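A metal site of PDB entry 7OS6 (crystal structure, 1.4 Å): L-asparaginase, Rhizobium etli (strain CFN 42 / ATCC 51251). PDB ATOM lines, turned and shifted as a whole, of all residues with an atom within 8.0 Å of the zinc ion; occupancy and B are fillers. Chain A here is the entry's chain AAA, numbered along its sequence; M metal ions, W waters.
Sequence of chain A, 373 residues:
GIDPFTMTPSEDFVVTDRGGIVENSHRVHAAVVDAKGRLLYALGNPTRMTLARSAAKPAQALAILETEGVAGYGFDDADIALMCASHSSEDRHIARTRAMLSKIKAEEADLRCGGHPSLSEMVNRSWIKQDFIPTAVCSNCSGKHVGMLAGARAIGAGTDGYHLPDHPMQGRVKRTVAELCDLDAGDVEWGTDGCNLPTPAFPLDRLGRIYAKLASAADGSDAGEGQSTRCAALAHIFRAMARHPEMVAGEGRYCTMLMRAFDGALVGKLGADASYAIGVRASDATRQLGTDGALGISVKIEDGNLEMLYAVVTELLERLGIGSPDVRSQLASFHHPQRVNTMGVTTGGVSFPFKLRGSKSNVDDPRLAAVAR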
ATOM      1  N   ARG A  53       1.127 -10.013   8.366  1.00  0.00           N
ATOM      2  CA  ARG A  53      -0.347 -10.198   8.346  1.00  0.00           C
ATOM      3  C   ARG A  53      -0.703 -10.935   7.046  1.00  0.00           C
ATOM      4  O   ARG A  53      -0.012 -11.927   6.681  1.00  0.00           O
ATOM      5  CB  ARG A  53      -0.995  -8.821   8.546  1.00  0.00           C
ATOM      6  CG  ARG A  53      -0.545  -8.097   9.813  1.00  0.00           C
ATOM      7  CD  ARG A  53      -1.017  -8.749  11.117  1.00  0.00           C
ATOM      8  NE  ARG A  53      -2.463  -8.720  11.238  1.00  0.00           N
ATOM      9  CZ  ARG A  53      -3.169  -7.633  11.509  1.00  0.00           C
ATOM     10  NH1 ARG A  53      -2.557  -6.476  11.730  1.00  0.00           N
ATOM     11  NH2 ARG A  53      -4.486  -7.698  11.533  1.00  0.00           N
ATOM     12  N   SER A  54      -1.713 -10.464   6.325  1.00  0.00           N
ATOM     13  CA  SER A  54      -2.194 -11.138   5.091  1.00  0.00           C
ATOM     14  C   SER A  54      -1.156 -11.159   4.013  1.00  0.00           C
ATOM     15  O   SER A  54      -1.310 -11.974   3.072  1.00  0.00           O
ATOM     16  CB  SER A  54      -3.463 -10.531   4.543  1.00  0.00           C
ATOM     17  OG  SER A  54      -4.529 -10.883   5.380  1.00  0.00           O
ATOM     18  N   LYS A  57       0.279 -14.564   3.200  1.00  0.00           N
ATOM     19  CA  LYS A  57      -0.629 -15.633   2.726  1.00  0.00           C
ATOM     20  C   LYS A  57       0.010 -16.513   1.640  1.00  0.00           C
ATOM     21  O   LYS A  57      -0.203 -17.719   1.683  1.00  0.00           O
ATOM     22  CB  LYS A  57      -1.974 -15.057   2.325  1.00  0.00           C
ATOM     23  CG  LYS A  57      -2.921 -14.865   3.493  1.00  0.00           C
ATOM     24  CD  LYS A  57      -4.161 -14.062   3.190  1.00  0.00           C
ATOM     25  CE  LYS A  57      -5.041 -13.934   4.403  1.00  0.00           C
ATOM     26  NZ  LYS A  57      -6.114 -12.936   4.200  1.00  0.00           N
ATOM     27  N   GLN A  60       1.890 -19.175   3.485  1.00  0.00           N
ATOM     28  CA  GLN A  60       0.918 -20.104   4.115  1.00  0.00           C
ATOM     29  C   GLN A  60       0.331 -21.035   3.062  1.00  0.00           C
ATOM     30  O   GLN A  60       0.217 -22.257   3.314  1.00  0.00           O
ATOM     31  CB  GLN A  60      -0.150 -19.329   4.895  1.00  0.00           C
ATOM     32  CG  GLN A  60       0.455 -18.684   6.136  1.00  0.00           C
ATOM     33  CD  GLN A  60      -0.358 -17.552   6.670  1.00  0.00           C
ATOM     34  OE1 GLN A  60      -0.637 -16.604   5.943  1.00  0.00           O
ATOM     35  NE2 GLN A  60      -0.764 -17.678   7.928  1.00  0.00           N
ATOM     36  N   MET A  83      -6.918 -18.949  -1.398  1.00  0.00           N
ATOM     37  CA  MET A  83      -5.987 -19.204  -0.251  1.00  0.00           C
ATOM     38  C   MET A  83      -5.069 -18.008  -0.036  1.00  0.00           C
ATOM     39  O   MET A  83      -4.780 -17.699   1.124  1.00  0.00           O
ATOM     40  CB  MET A  83      -5.097 -20.417  -0.499  1.00  0.00           C
ATOM     41  CG  MET A  83      -5.864 -21.683  -0.591  1.00  0.00           C
ATOM     42  SD  MET A  83      -4.632 -23.037  -0.780  1.00  0.00           S
ATOM     43  CE  MET A  83      -5.774 -24.323  -1.291  1.00  0.00           C
ATOM     44  N   ALA A  85      -5.860 -14.856  -0.574  1.00  0.00           N
ATOM     45  CA  ALA A  85      -6.735 -13.653  -0.613  1.00  0.00           C
ATOM     46  C   ALA A  85      -6.920 -12.973   0.745  1.00  0.00           C
ATOM     47  O   ALA A  85      -7.025 -13.654   1.781  1.00  0.00           O
ATOM     48  CB  ALA A  85      -8.104 -14.049  -1.099  1.00  0.00           C
ATOM     49  N   SER A  86      -7.159 -11.671   0.703  1.00  0.00           N
ATOM     50  CA  SER A  86      -7.963 -10.903   1.704  1.00  0.00           C
ATOM     51  C   SER A  86      -9.190 -10.405   0.968  1.00  0.00           C
ATOM     52  O   SER A  86      -9.262  -9.263   0.498  1.00  0.00           O
ATOM     53  CB  SER A  86      -7.228  -9.752   2.313  1.00  0.00           C
ATOM     54  OG  SER A  86      -6.044 -10.209   2.976  1.00  0.00           O
ATOM     55  N   CYS A 113     -12.079 -19.464  11.944  1.00  0.00           N
ATOM     56  CA  CYS A 113     -12.112 -17.995  11.734  1.00  0.00           C
ATOM     57  C   CYS A 113     -13.533 -17.485  11.963  1.00  0.00           C
ATOM     58  O   CYS A 113     -14.511 -18.283  11.887  1.00  0.00           O
ATOM     59  CB  CYS A 113     -11.628 -17.640  10.336  1.00  0.00           C
ATOM     60  SG  CYS A 113     -12.471 -18.513   8.966  1.00  0.00           S
ATOM     61  N   SER A 139     -15.308 -14.767   6.193  1.00  0.00           N
ATOM     62  CA  SER A 139     -13.984 -14.207   6.574  1.00  0.00           C
ATOM     63  C   SER A 139     -13.187 -13.906   5.308  1.00  0.00           C
ATOM     64  O   SER A 139     -13.066 -14.747   4.424  1.00  0.00           O
ATOM     65  CB  SER A 139     -13.267 -15.167   7.437  1.00  0.00           C
ATOM     66  OG  SER A 139     -11.916 -14.748   7.643  1.00  0.00           O
ATOM     67  N   ASN A 140     -12.491 -12.772   5.308  1.00  0.00           N
ATOM     68  CA  ASN A 140     -11.516 -12.427   4.242  1.00  0.00           C
ATOM     69  C   ASN A 140     -10.434 -13.508   4.138  1.00  0.00           C
ATOM     70  O   ASN A 140      -9.844 -13.612   3.043  1.00  0.00           O
ATOM     71  CB  ASN A 140     -10.914 -11.025   4.454  1.00  0.00           C
ATOM     72  CG  ASN A 140      -9.766 -11.024   5.458  1.00  0.00           C
ATOM     73  OD1 ASN A 140      -8.574 -11.035   5.090  1.00  0.00           O
ATOM     74  ND2 ASN A 140     -10.102 -11.073   6.720  1.00  0.00           N
ATOM     75  N   CYS A 141     -10.197 -14.260   5.229  1.00  0.00           N
ATOM     76  CA  CYS A 141      -9.180 -15.324   5.308  1.00  0.00           C
ATOM     77  C   CYS A 141      -9.797 -16.708   5.093  1.00  0.00           C
ATOM     78  O   CYS A 141      -9.116 -17.703   5.357  1.00  0.00           O
ATOM     79  CB  CYS A 141      -8.488 -15.322   6.662  1.00  0.00           C
ATOM     80  SG  CYS A 141      -7.533 -13.799   6.945  1.00  0.00           S
ATOM     81  N   SER A 142     -11.071 -16.764   4.674  1.00  0.00           N
ATOM     82  CA  SER A 142     -11.772 -18.064   4.564  1.00  0.00           C
ATOM     83  C   SER A 142     -10.980 -19.057   3.685  1.00  0.00           C
ATOM     84  O   SER A 142     -10.945 -20.256   4.019  1.00  0.00           O
ATOM     85  CB  SER A 142     -13.191 -17.897   4.092  1.00  0.00           C
ATOM     86  OG  SER A 142     -13.213 -17.384   2.776  1.00  0.00           O
ATOM     87  N   LYS A 144      -7.677 -19.343   3.073  1.00  0.00           N
ATOM     88  CA  LYS A 144      -6.513 -19.827   3.853  1.00  0.00           C
ATOM     89  C   LYS A 144      -6.987 -20.848   4.875  1.00  0.00           C
ATOM     90  O   LYS A 144      -6.372 -21.916   5.027  1.00  0.00           O
ATOM     91  CB  LYS A 144      -5.843 -18.637   4.526  1.00  0.00           C
ATOM     92  CG  LYS A 144      -4.799 -19.021   5.544  1.00  0.00           C
ATOM     93  CD  LYS A 144      -4.047 -17.830   6.172  1.00  0.00           C
ATOM     94  CE  LYS A 144      -5.048 -16.882   6.782  1.00  0.00           C
ATOM     95  NZ  LYS A 144      -4.407 -15.792   7.573  1.00  0.00           N
ATOM     96  N   HIS A 145      -8.080 -20.570   5.578  1.00  0.00           N
ATOM     97  CA  HIS A 145      -8.601 -21.484   6.632  1.00  0.00           C
ATOM     98  C   HIS A 145      -9.056 -22.809   5.997  1.00  0.00           C
ATOM     99  O   HIS A 145      -8.763 -23.858   6.558  1.00  0.00           O
ATOM    100  CB  HIS A 145      -9.709 -20.823   7.415  1.00  0.00           C
ATOM    101  CG  HIS A 145      -9.181 -19.950   8.493  1.00  0.00           C
ATOM    102  ND1 HIS A 145      -9.143 -20.371   9.798  1.00  0.00           N
ATOM    103  CD2 HIS A 145      -8.603 -18.725   8.450  1.00  0.00           C
ATOM    104  CE1 HIS A 145      -8.589 -19.411  10.527  1.00  0.00           C
ATOM    105  NE2 HIS A 145      -8.291 -18.386   9.743  1.00  0.00           N
ATOM    106  N   ASP A 193      -3.546 -13.600  14.617  1.00  0.00           N
ATOM    107  CA  ASP A 193      -4.178 -12.708  13.617  1.00  0.00           C
ATOM    108  C   ASP A 193      -5.652 -12.489  13.955  1.00  0.00           C
ATOM    109  O   ASP A 193      -6.221 -13.146  14.862  1.00  0.00           O
ATOM    110  CB  ASP A 193      -3.993 -13.302  12.223  1.00  0.00           C
ATOM    111  CG  ASP A 193      -3.537 -12.350  11.174  1.00  0.00           C
ATOM    112  OD1 ASP A 193      -3.906 -11.188  11.299  1.00  0.00           O
ATOM    113  OD2 ASP A 193      -2.905 -12.840  10.177  1.00  0.00           O
ATOM    114  N   GLY A 194      -6.286 -11.582  13.208  1.00  0.00           N
ATOM    115  CA  GLY A 194      -7.722 -11.315  13.342  1.00  0.00           C
ATOM    116  C   GLY A 194      -8.553 -12.541  13.029  1.00  0.00           C
ATOM    117  O   GLY A 194      -9.596 -12.684  13.638  1.00  0.00           O
ATOM    118  N   CYS A 195      -8.050 -13.402  12.173  1.00  0.00           N
ATOM    119  CA  CYS A 195      -8.723 -14.668  11.744  1.00  0.00           C
ATOM    120  C   CYS A 195      -8.388 -15.833  12.680  1.00  0.00           C
ATOM    121  O   CYS A 195      -8.839 -16.979  12.423  1.00  0.00           O
ATOM    122  CB  CYS A 195      -8.356 -15.012  10.305  1.00  0.00           C
ATOM    123  SG  CYS A 195      -6.600 -15.479  10.220  1.00  0.00           S
ATOM    124  N   ASN A 196      -7.643 -15.592  13.764  1.00  0.00           N
ATOM    125  CA  ASN A 196      -7.370 -16.534  14.866  1.00  0.00           C
ATOM    126  C   ASN A 196      -6.308 -17.583  14.475  1.00  0.00           C
ATOM    127  O   ASN A 196      -6.205 -18.604  15.184  1.00  0.00           O
ATOM    128  CB  ASN A 196      -8.645 -17.248  15.313  1.00  0.00           C
ATOM    129  CG  ASN A 196      -8.579 -17.623  16.758  1.00  0.00           C
ATOM    130  OD1 ASN A 196      -7.972 -16.956  17.595  1.00  0.00           O
ATOM    131  ND2 ASN A 196      -9.241 -18.716  17.080  1.00  0.00           N
ATOM    132  N   LEU A 197      -5.475 -17.329  13.485  1.00  0.00           N
ATOM    133  CA  LEU A 197      -4.290 -18.161  13.168  1.00  0.00           C
ATOM    134  C   LEU A 197      -3.031 -17.499  13.697  1.00  0.00           C
ATOM    135  O   LEU A 197      -2.974 -16.268  13.803  1.00  0.00           O
ATOM    136  CB  LEU A 197      -4.139 -18.317  11.662  1.00  0.00           C
ATOM    137  CG  LEU A 197      -5.082 -19.324  11.012  1.00  0.00           C
ATOM    138  CD1 LEU A 197      -5.099 -19.179   9.509  1.00  0.00           C
ATOM    139  CD2 LEU A 197      -4.636 -20.731  11.370  1.00  0.00           C
ATOM    140  N   PRO A 198      -1.945 -18.272  13.909  1.00  0.00           N
ATOM    141  CA  PRO A 198      -0.618 -17.680  14.130  1.00  0.00           C
ATOM    142  C   PRO A 198      -0.247 -16.819  12.926  1.00  0.00           C
ATOM    143  O   PRO A 198      -0.561 -17.158  11.787  1.00  0.00           O
ATOM    144  CB  PRO A 198       0.309 -18.897  14.206  1.00  0.00           C
ATOM    145  CG  PRO A 198      -0.604 -20.033  14.601  1.00  0.00           C
ATOM    146  CD  PRO A 198      -1.896 -19.745  13.878  1.00  0.00           C
ATOM    147  N   THR A 199       0.408 -15.690  13.200  1.00  0.00           N
ATOM    148  CA  THR A 199       0.808 -14.701  12.172  1.00  0.00           C
ATOM    149  C   THR A 199       2.244 -14.275  12.437  1.00  0.00           C
ATOM    150  O   THR A 199       2.574 -13.996  13.591  1.00  0.00           O
ATOM    151  CB  THR A 199      -0.248 -13.587  12.112  1.00  0.00           C
ATOM    152  OG1 THR A 199      -0.046 -12.915  10.875  1.00  0.00           O
ATOM    153  CG2 THR A 199      -0.217 -12.622  13.275  1.00  0.00           C
HETATM  154 ZN    ZN M   1      -5.862 -14.437   8.320  1.00  0.00          ZN
HETATM  155  O   HOH W   1      -4.751 -12.683   8.287  1.00  0.00           O
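The side-chain sulfur (SG) of Cys 141 lies close to the side-chain amino group (NZ) of Lys 57. The side-chain sulfur of Cys 141 sits close to the side-chain amide oxygen of Asn 140. The side-chain hydroxyl (OG) of Ser 139 is in hydrogen-bond range of the backbone NH (N) of Cys 141 (3.0 Å). O of Cys 195 is in hydrogen-bond range of NE2 of His 145 (3.1 Å). The guanidinium group (NE) of Arg 53 is in salt-bridge range of the side-chain carboxylate (OD1) of Asp 193, 2.9 Å away. OD2 of Asp 193 lies within hydrogen-bond range of OG1 of Thr 199 (2.9 Å).
OD2 of Asp 193 touches the zinc ion (3.8 Å). Of the 21 residues printed, 4 come within 4 Å of the zinc ion. The nearest printed residue that does not touch the zinc ion is Lys 57 (4.03 Å).
Water W1 is bound to the zinc ion. NZ of Lys 144 is bound to the zinc ion, at 2.1 Å. SG of Cys 141 binds the zinc ion. The zinc ion is bound by the side-chain sulfur (SG) of Cys 195 (2.3 Å). The zinc ion has four donor atoms within binding distance.
Water W1 bridges the side-chain carboxylate of Asp 193 (2.6 Å) and the side-chain hydroxyl of Ser 54 (3.4 Å).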
